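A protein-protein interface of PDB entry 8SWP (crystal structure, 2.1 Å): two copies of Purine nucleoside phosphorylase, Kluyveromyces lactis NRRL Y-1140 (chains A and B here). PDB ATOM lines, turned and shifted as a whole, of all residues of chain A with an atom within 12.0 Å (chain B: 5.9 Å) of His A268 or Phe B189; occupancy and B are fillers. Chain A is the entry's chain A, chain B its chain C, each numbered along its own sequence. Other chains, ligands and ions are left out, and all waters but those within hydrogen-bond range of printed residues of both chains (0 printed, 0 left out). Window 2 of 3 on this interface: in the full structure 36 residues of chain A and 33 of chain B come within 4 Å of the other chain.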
ATOM      1  N   PRO A 263      -1.493 -29.696  12.665  1.00  0.00           N
ATOM      2  CA  PRO A 263      -2.324 -30.049  13.812  1.00  0.00           C
ATOM      3  C   PRO A 263      -3.766 -29.660  13.562  1.00  0.00           C
ATOM      4  O   PRO A 263      -4.049 -28.689  12.835  1.00  0.00           O
ATOM      5  CB  PRO A 263      -1.708 -29.235  14.960  1.00  0.00           C
ATOM      6  CG  PRO A 263      -0.860 -28.192  14.306  1.00  0.00           C
ATOM      7  CD  PRO A 263      -0.384 -28.801  13.032  1.00  0.00           C
ATOM      8  N   PRO A 264      -4.715 -30.395  14.136  1.00  0.00           N
ATOM      9  CA  PRO A 264      -6.129 -30.102  13.885  1.00  0.00           C
ATOM     10  C   PRO A 264      -6.530 -28.769  14.498  1.00  0.00           C
ATOM     11  O   PRO A 264      -5.816 -28.178  15.311  1.00  0.00           O
ATOM     12  CB  PRO A 264      -6.860 -31.272  14.549  1.00  0.00           C
ATOM     13  CG  PRO A 264      -5.928 -31.735  15.614  1.00  0.00           C
ATOM     14  CD  PRO A 264      -4.534 -31.491  15.104  1.00  0.00           C
ATOM     15  N   ALA A 265      -7.700 -28.293  14.079  1.00  0.00           N
ATOM     16  CA  ALA A 265      -8.214 -27.025  14.575  1.00  0.00           C
ATOM     17  C   ALA A 265      -8.391 -27.075  16.086  1.00  0.00           C
ATOM     18  O   ALA A 265      -8.974 -28.019  16.626  1.00  0.00           O
ATOM     19  CB  ALA A 265      -9.543 -26.693  13.896  1.00  0.00           C
ATOM     20  N   SER A 266      -7.870 -26.059  16.768  1.00  0.00           N
ATOM     21  CA  SER A 266      -8.019 -25.971  18.210  1.00  0.00           C
ATOM     22  C   SER A 266      -9.403 -25.436  18.569  1.00  0.00           C
ATOM     23  O   SER A 266     -10.054 -24.741  17.785  1.00  0.00           O
ATOM     24  CB  SER A 266      -6.935 -25.076  18.810  1.00  0.00           C
ATOM     25  OG  SER A 266      -7.206 -24.785  20.170  1.00  0.00           O
ATOM     26  N   ALA A 267      -9.851 -25.776  19.780  1.00  0.00           N
ATOM     27  CA  ALA A 267     -11.172 -25.346  20.221  1.00  0.00           C
ATOM     28  C   ALA A 267     -11.237 -23.840  20.437  1.00  0.00           C
ATOM     29  O   ALA A 267     -12.315 -23.246  20.327  1.00  0.00           O
ATOM     30  CB  ALA A 267     -11.565 -26.082  21.502  1.00  0.00           C
ATOM     31  N   HIS A 268     -10.103 -23.207  20.738  1.00  0.00           N
ATOM     32  CA  HIS A 268     -10.045 -21.771  20.975  1.00  0.00           C
ATOM     33  C   HIS A 268      -9.652 -20.989  19.727  1.00  0.00           C
ATOM     34  O   HIS A 268      -9.265 -19.820  19.831  1.00  0.00           O
ATOM     35  CB  HIS A 268      -9.086 -21.465  22.125  1.00  0.00           C
ATOM     36  CG  HIS A 268      -8.959 -22.581  23.115  1.00  0.00           C
ATOM     37  ND1 HIS A 268      -9.890 -22.806  24.106  1.00  0.00           N
ATOM     38  CD2 HIS A 268      -8.011 -23.536  23.266  1.00  0.00           C
ATOM     39  CE1 HIS A 268      -9.521 -23.851  24.824  1.00  0.00           C
ATOM     40  NE2 HIS A 268      -8.384 -24.312  24.336  1.00  0.00           N
ATOM     41  N   ASP A 269      -9.740 -21.608  18.553  1.00  0.00           N
ATOM     42  CA  ASP A 269      -9.572 -20.904  17.288  1.00  0.00           C
ATOM     43  C   ASP A 269     -10.944 -20.464  16.794  1.00  0.00           C
ATOM     44  O   ASP A 269     -11.822 -21.303  16.565  1.00  0.00           O
ATOM     45  CB  ASP A 269      -8.890 -21.794  16.249  1.00  0.00           C
ATOM     46  CG  ASP A 269      -7.467 -22.156  16.629  1.00  0.00           C
ATOM     47  OD1 ASP A 269      -6.848 -21.409  17.415  1.00  0.00           O
ATOM     48  OD2 ASP A 269      -6.964 -23.187  16.133  1.00  0.00           O
ATOM     49  N   GLU A 270     -11.135 -19.156  16.642  1.00  0.00           N
ATOM     50  CA  GLU A 270     -12.383 -18.635  16.101  1.00  0.00           C
ATOM     51  C   GLU A 270     -12.330 -18.436  14.592  1.00  0.00           C
ATOM     52  O   GLU A 270     -13.289 -17.914  14.014  1.00  0.00           O
ATOM     53  CB  GLU A 270     -12.759 -17.320  16.796  1.00  0.00           C
ATOM     54  CG  GLU A 270     -11.705 -16.233  16.738  1.00  0.00           C
ATOM     55  CD  GLU A 270     -12.144 -14.972  17.460  1.00  0.00           C
ATOM     56  OE1 GLU A 270     -13.312 -14.918  17.904  1.00  0.00           O
ATOM     57  OE2 GLU A 270     -11.324 -14.039  17.589  1.00  0.00           O
ATOM     58  N   ASN A 271     -11.238 -18.839  13.947  1.00  0.00           N
ATOM     59  CA  ASN A 271     -11.158 -18.930  12.488  1.00  0.00           C
ATOM     60  C   ASN A 271     -10.620 -20.306  12.105  1.00  0.00           C
ATOM     61  O   ASN A 271      -9.567 -20.426  11.472  1.00  0.00           O
ATOM     62  CB  ASN A 271     -10.283 -17.813  11.921  1.00  0.00           C
ATOM     63  CG  ASN A 271      -8.907 -17.765  12.560  1.00  0.00           C
ATOM     64  OD1 ASN A 271      -8.676 -18.371  13.606  1.00  0.00           O
ATOM     65  ND2 ASN A 271      -7.985 -17.044  11.931  1.00  0.00           N
ATOM     66  N   PRO A 272     -11.332 -21.372  12.467  1.00  0.00           N
ATOM     67  CA  PRO A 272     -10.749 -22.712  12.363  1.00  0.00           C
ATOM     68  C   PRO A 272     -10.869 -23.287  10.962  1.00  0.00           C
ATOM     69  O   PRO A 272     -11.882 -23.118  10.280  1.00  0.00           O
ATOM     70  CB  PRO A 272     -11.573 -23.538  13.363  1.00  0.00           C
ATOM     71  CG  PRO A 272     -12.725 -22.640  13.811  1.00  0.00           C
ATOM     72  CD  PRO A 272     -12.725 -21.427  12.934  1.00  0.00           C
ATOM     73  N   VAL A 273      -9.817 -23.971  10.540  1.00  0.00           N
ATOM     74  CA  VAL A 273      -9.872 -24.769   9.315  1.00  0.00           C
ATOM     75  C   VAL A 273     -10.606 -26.072   9.622  1.00  0.00           C
ATOM     76  O   VAL A 273     -10.278 -26.736  10.618  1.00  0.00           O
ATOM     77  CB  VAL A 273      -8.465 -25.041   8.789  1.00  0.00           C
ATOM     78  CG1 VAL A 273      -8.512 -25.975   7.588  1.00  0.00           C
ATOM     79  CG2 VAL A 273      -7.776 -23.733   8.427  1.00  0.00           C
ATOM     80  N   ILE A 275     -11.642 -29.697  10.246  1.00  0.00           N
ATOM     81  CA  ILE A 275     -10.804 -30.869  10.472  1.00  0.00           C
ATOM     82  C   ILE A 275     -10.959 -31.899   9.363  1.00  0.00           C
ATOM     83  O   ILE A 275     -10.059 -32.716   9.147  1.00  0.00           O
ATOM     84  CB  ILE A 275     -11.122 -31.491  11.847  1.00  0.00           C
ATOM     85  CG1 ILE A 275     -12.557 -32.023  11.874  1.00  0.00           C
ATOM     86  CG2 ILE A 275     -10.905 -30.475  12.956  1.00  0.00           C
ATOM     87  CD1 ILE A 275     -12.867 -32.885  13.074  1.00  0.00           C
ATOM     88  N   CYS B 145      -8.379 -32.576  26.774  1.00  0.00           N
ATOM     89  CA  CYS B 145      -9.312 -32.871  25.695  1.00  0.00           C
ATOM     90  C   CYS B 145      -8.532 -33.397  24.496  1.00  0.00           C
ATOM     91  O   CYS B 145      -7.699 -32.682  23.928  1.00  0.00           O
ATOM     92  CB  CYS B 145     -10.110 -31.623  25.328  1.00  0.00           C
ATOM     93  SG  CYS B 145     -11.080 -31.789  23.822  1.00  0.00           S
ATOM     94  N   LEU B 184     -17.728 -30.573  19.217  1.00  0.00           N
ATOM     95  CA  LEU B 184     -17.940 -31.270  20.510  1.00  0.00           C
ATOM     96  C   LEU B 184     -16.879 -30.786  21.496  1.00  0.00           C
ATOM     97  O   LEU B 184     -17.174 -30.726  22.693  1.00  0.00           O
ATOM     98  CB  LEU B 184     -17.870 -32.782  20.296  1.00  0.00           C
ATOM     99  CG  LEU B 184     -19.107 -33.415  19.668  1.00  0.00           C
ATOM    100  CD1 LEU B 184     -18.906 -34.909  19.486  1.00  0.00           C
ATOM    101  CD2 LEU B 184     -20.339 -33.141  20.516  1.00  0.00           C
ATOM    102  N   ARG B 185     -15.705 -30.420  20.985  1.00  0.00           N
ATOM    103  CA  ARG B 185     -14.609 -29.925  21.850  1.00  0.00           C
ATOM    104  C   ARG B 185     -14.954 -28.505  22.276  1.00  0.00           C
ATOM    105  O   ARG B 185     -14.778 -28.184  23.455  1.00  0.00           O
ATOM    106  CB  ARG B 185     -13.272 -29.976  21.107  1.00  0.00           C
ATOM    107  CG  ARG B 185     -12.820 -31.383  20.742  1.00  0.00           C
ATOM    108  CD  ARG B 185     -11.419 -31.445  20.166  1.00  0.00           C
ATOM    109  NE  ARG B 185     -11.414 -31.479  18.712  1.00  0.00           N
ATOM    110  CZ  ARG B 185     -10.794 -30.591  17.947  1.00  0.00           C
ATOM    111  NH1 ARG B 185     -10.111 -29.607  18.500  1.00  0.00           N
ATOM    112  NH2 ARG B 185     -10.854 -30.694  16.633  1.00  0.00           N
ATOM    113  N   LYS B 186     -15.453 -27.708  21.337  1.00  0.00           N
ATOM    114  CA  LYS B 186     -15.875 -26.326  21.677  1.00  0.00           C
ATOM    115  C   LYS B 186     -17.000 -26.412  22.716  1.00  0.00           C
ATOM    116  O   LYS B 186     -16.973 -25.631  23.674  1.00  0.00           O
ATOM    117  CB  LYS B 186     -16.251 -25.559  20.405  1.00  0.00           C
ATOM    118  CG  LYS B 186     -15.081 -25.181  19.509  1.00  0.00           C
ATOM    119  CD  LYS B 186     -15.506 -24.738  18.130  1.00  0.00           C
ATOM    120  CE  LYS B 186     -14.845 -23.450  17.691  1.00  0.00           C
ATOM    121  NZ  LYS B 186     -13.371 -23.577  17.628  1.00  0.00           N
ATOM    122  N   LEU B 187     -17.908 -27.370  22.567  1.00  0.00           N
ATOM    123  CA  LEU B 187     -18.990 -27.559  23.565  1.00  0.00           C
ATOM    124  C   LEU B 187     -18.378 -27.821  24.941  1.00  0.00           C
ATOM    125  O   LEU B 187     -18.774 -27.151  25.899  1.00  0.00           O
ATOM    126  CB  LEU B 187     -19.870 -28.730  23.131  1.00  0.00           C
ATOM    127  CG  LEU B 187     -21.029 -29.070  24.065  1.00  0.00           C
ATOM    128  CD1 LEU B 187     -21.937 -27.868  24.260  1.00  0.00           C
ATOM    129  CD2 LEU B 187     -21.824 -30.252  23.532  1.00  0.00           C
ATOM    130  N   LEU B 188     -17.442 -28.759  25.026  1.00  0.00           N
ATOM    131  CA  LEU B 188     -16.874 -29.124  26.349  1.00  0.00           C
ATOM    132  C   LEU B 188     -16.270 -27.882  26.997  1.00  0.00           C
ATOM    133  O   LEU B 188     -16.519 -27.658  28.191  1.00  0.00           O
ATOM    134  CB  LEU B 188     -15.812 -30.210  26.169  1.00  0.00           C
ATOM    135  CG  LEU B 188     -15.117 -30.663  27.449  1.00  0.00           C
ATOM    136  CD1 LEU B 188     -15.935 -31.733  28.148  1.00  0.00           C
ATOM    137  CD2 LEU B 188     -13.718 -31.171  27.151  1.00  0.00           C
ATOM    138  N   PHE B 189     -15.524 -27.102  26.227  1.00  0.00           N
ATOM    139  CA  PHE B 189     -14.844 -25.932  26.825  1.00  0.00           C
ATOM    140  C   PHE B 189     -15.903 -24.930  27.304  1.00  0.00           C
ATOM    141  O   PHE B 189     -15.714 -24.328  28.371  1.00  0.00           O
ATOM    142  CB  PHE B 189     -13.818 -25.374  25.838  1.00  0.00           C
ATOM    143  CG  PHE B 189     -12.521 -26.147  25.838  1.00  0.00           C
ATOM    144  CD1 PHE B 189     -11.617 -26.016  26.880  1.00  0.00           C
ATOM    145  CD2 PHE B 189     -12.217 -27.032  24.819  1.00  0.00           C
ATOM    146  CE1 PHE B 189     -10.432 -26.736  26.888  1.00  0.00           C
ATOM    147  CE2 PHE B 189     -11.033 -27.753  24.829  1.00  0.00           C
ATOM    148  CZ  PHE B 189     -10.142 -27.603  25.863  1.00  0.00           C
ATOM    149  N   SER B 190     -16.989 -24.782  26.545  1.00  0.00           N
ATOM    150  CA  SER B 190     -18.078 -23.846  26.929  1.00  0.00           C
ATOM    151  C   SER B 190     -18.694 -24.310  28.244  1.00  0.00           C
ATOM    152  O   SER B 190     -18.963 -23.466  29.097  1.00  0.00           O
ATOM    153  CB  SER B 190     -19.106 -23.765  25.854  1.00  0.00           C
ATOM    154  OG  SER B 190     -20.068 -24.796  26.001  1.00  0.00           O
ATOM    155  N   LYS B 191     -18.846 -25.617  28.405  1.00  0.00           N
ATOM    156  CA  LYS B 191     -19.516 -26.145  29.616  1.00  0.00           C
ATOM    157  C   LYS B 191     -18.619 -25.936  30.842  1.00  0.00           C
ATOM    158  O   LYS B 191     -19.153 -25.700  31.920  1.00  0.00           O
ATOM    159  CB  LYS B 191     -19.925 -27.595  29.356  1.00  0.00           C
ATOM    160  CG  LYS B 191     -21.058 -27.774  28.356  1.00  0.00           C
ATOM    161  CD  LYS B 191     -22.038 -26.626  28.377  1.00  0.00           C
ATOM    162  CE  LYS B 191     -23.428 -27.015  27.922  1.00  0.00           C
ATOM    163  NZ  LYS B 191     -24.223 -25.828  27.529  1.00  0.00           N
ATOM    164  N   LYS B 192     -17.302 -25.961  30.665  1.00  0.00           N
ATOM    165  CA  LYS B 192     -16.368 -25.742  31.797  1.00  0.00           C
ATOM    166  C   LYS B 192     -16.533 -24.310  32.301  1.00  0.00           C
ATOM    167  O   LYS B 192     -16.604 -24.123  33.522  1.00  0.00           O
ATOM    168  CB  LYS B 192     -14.931 -26.011  31.354  1.00  0.00           C
ATOM    169  CG  LYS B 192     -13.842 -25.572  32.323  1.00  0.00           C
ATOM    170  CD  LYS B 192     -12.921 -24.526  31.738  1.00  0.00           C
ATOM    171  CE  LYS B 192     -11.462 -24.761  32.064  1.00  0.00           C
ATOM    172  NZ  LYS B 192     -11.262 -25.069  33.499  1.00  0.00           N
ATOM    173  N   LYS B 193     -16.580 -23.347  31.385  1.00  0.00           N
ATOM    174  CA  LYS B 193     -16.773 -21.926  31.767  1.00  0.00           C
ATOM    175  C   LYS B 193     -18.123 -21.772  32.472  1.00  0.00           C
ATOM    176  O   LYS B 193     -18.147 -21.176  33.551  1.00  0.00           O
ATOM    177  CB  LYS B 193     -16.702 -21.044  30.520  1.00  0.00           C
ATOM    178  CG  LYS B 193     -16.522 -19.558  30.780  1.00  0.00           C
ATOM    179  CD  LYS B 193     -17.305 -18.693  29.818  1.00  0.00           C
ATOM    180  CE  LYS B 193     -16.446 -17.683  29.087  1.00  0.00           C
ATOM    181  NZ  LYS B 193     -16.876 -17.515  27.679  1.00  0.00           N
ATOM    182  N   GLU B 194     -19.188 -22.312  31.885  1.00  0.00           N
ATOM    183  CA  GLU B 194     -20.527 -22.263  32.513  1.00  0.00           C
ATOM    184  C   GLU B 194     -20.460 -22.842  33.921  1.00  0.00           C
ATOM    185  O   GLU B 194     -21.032 -22.225  34.824  1.00  0.00           O
ATOM    186  CB  GLU B 194     -21.517 -23.113  31.723  1.00  0.00           C
ATOM    187  CG  GLU B 194     -21.953 -22.510  30.404  1.00  0.00           C
ATOM    188  CD  GLU B 194     -22.980 -23.358  29.676  1.00  0.00           C
ATOM    189  OE1 GLU B 194     -23.676 -24.143  30.345  1.00  0.00           O
ATOM    190  OE2 GLU B 194     -23.076 -23.239  28.440  1.00  0.00           O
ATOM    191  N   ILE B 201      -7.991 -27.768  31.619  1.00  0.00           N
ATOM    192  CA  ILE B 201      -8.336 -28.771  30.579  1.00  0.00           C
ATOM    193  C   ILE B 201      -7.451 -28.467  29.375  1.00  0.00           C
ATOM    194  O   ILE B 201      -7.606 -27.390  28.787  1.00  0.00           O
ATOM    195  CB  ILE B 201      -9.823 -28.713  30.202  1.00  0.00           C
ATOM    196  CG1 ILE B 201     -10.721 -28.765  31.438  1.00  0.00           C
ATOM    197  CG2 ILE B 201     -10.166 -29.813  29.211  1.00  0.00           C
ATOM    198  CD1 ILE B 201     -12.184 -28.853  31.111  1.00  0.00           C
ATOM    199  N   HIS B 202      -6.552 -29.393  29.047  1.00  0.00           N
ATOM    200  CA  HIS B 202      -5.624 -29.182  27.912  1.00  0.00           C
ATOM    201  C   HIS B 202      -6.223 -29.760  26.634  1.00  0.00           C
ATOM    202  O   HIS B 202      -7.217 -30.473  26.714  1.00  0.00           O
ATOM    203  CB  HIS B 202      -4.291 -29.867  28.209  1.00  0.00           C
ATOM    204  CG  HIS B 202      -3.622 -29.427  29.464  1.00  0.00           C
ATOM    205  ND1 HIS B 202      -2.863 -28.281  29.532  1.00  0.00           N
ATOM    206  CD2 HIS B 202      -3.565 -29.985  30.674  1.00  0.00           C
ATOM    207  CE1 HIS B 202      -2.382 -28.154  30.757  1.00  0.00           C
ATOM    208  NE2 HIS B 202      -2.796 -29.177  31.466  1.00  0.00           N
ATOM    209  N   GLU B 203      -5.656 -29.406  25.491  1.00  0.00           N
ATOM    210  CA  GLU B 203      -6.069 -30.026  24.211  1.00  0.00           C
ATOM    211  C   GLU B 203      -4.812 -30.705  23.665  1.00  0.00           C
ATOM    212  O   GLU B 203      -3.844 -29.988  23.393  1.00  0.00           O
ATOM    213  CB  GLU B 203      -6.627 -28.976  23.252  1.00  0.00           C
ATOM    214  CG  GLU B 203      -7.755 -29.474  22.372  1.00  0.00           C
ATOM    215  CD  GLU B 203      -8.357 -28.397  21.483  1.00  0.00           C
ATOM    216  OE1 GLU B 203      -7.758 -27.312  21.385  1.00  0.00           O
ATOM    217  OE2 GLU B 203      -9.419 -28.649  20.892  1.00  0.00           O
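Among the printed residues, pairs that only touch across the chains: Ala A267 with Phe B189 (3.5 Å), Ser A266 with Lys B186 (3.5 Å), His A268 with Phe B189 (3.6 Å), Ile A275 with Arg B185 (3.7 Å) and Pro A272 with Lys B186 (3.98 Å).
Of the 15 printed residues of chain B, 4 touch a printed residue of chain A.
Hydrophobic or aromatic side chains of chain B that line the printed part of chain A: Phe B189.
Printed residues of chain A that touch a printed residue of chain B: Ala A265, Ser A266, Ala A267, His A268, Asp A269, Pro A272 and Ile A275.
Hydrophobic or aromatic side chains of chain A within 4 Å of the printed part of chain B: Ala A267, His A268, Pro A272 and Ile A275.
Among the printed residues, no Asp or Glu carboxylate lies within 4 Å of a Lys or Arg side-chain nitrogen of the other chain.
The side-chain hydroxyl (OG) of Ser A266 is in hydrogen-bond range of the side-chain carboxylate (OE1) of Glu B203, at 2.9 Å.
The backbone NH of Ala A267 lies within hydrogen-bond range of the side-chain carboxylate of Glu B203, 3.1 Å away.
O of Ala A265 lies within hydrogen-bond range of NH1 of Arg B185 (2.7 Å).
The backbone carbonyl oxygen of Ala A267 lies within hydrogen-bond range of the side-chain amino group of Lys B186.
The backbone carbonyl oxygen (O) of Asp A269 is in hydrogen-bond range of the side-chain amino group (NZ) of Lys B186 (2.9 Å).
The backbone NH (N) of His A268 sits close to the side-chain hydroxyl (OG) of Ser A266 (3.3 Å).
NH1 of Arg B185 lies within salt-bridge range of OE2 of Glu B203 (2.7 Å).
The backbone NH (N) of Ser A266 lies within hydrogen-bond range of the side-chain carboxylate (OD2) of Asp A269 (3.1 Å).
Printed residues of chain B within 4 Å of Ala A265: Arg B185.
Printed residues of chain B within 4 Å of Ser A266: Lys B186 (3.5 Å) and Glu B203 (2.9 Å).
Of the printed residues of chain B, Ala A267 touches Lys B186 (2.9 Å), Phe B189 (3.5 Å) and Glu B203 (3.1 Å).
His A268 touches one residue of chain B.
Val A273 touches none of the printed residues of chain B.
No residue of chain A comes within 4 Å of Cys B145.
No residue of chain A comes within 4 Å of Leu B188.
Phe B189 touches just these residues of chain A: Ala A267 (3.5 Å) and His A268 (3.6 Å).
No residue of chain A comes within 4 Å of Ser B190.
No residue of chain A comes within 4 Å of Lys B193.
Glu B203 touches just these residues of chain A: Ser A266 (2.9 Å) and Ala A267 (3.1 Å).
The nearest printed residue of chain A that does not touch Lys B186 is His A268 (4.5 Å).
No position is printed for both chains.
Of the 10 pairs that touch across the chains among the printed residues, none has its exchanged pair printed and touching as well.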
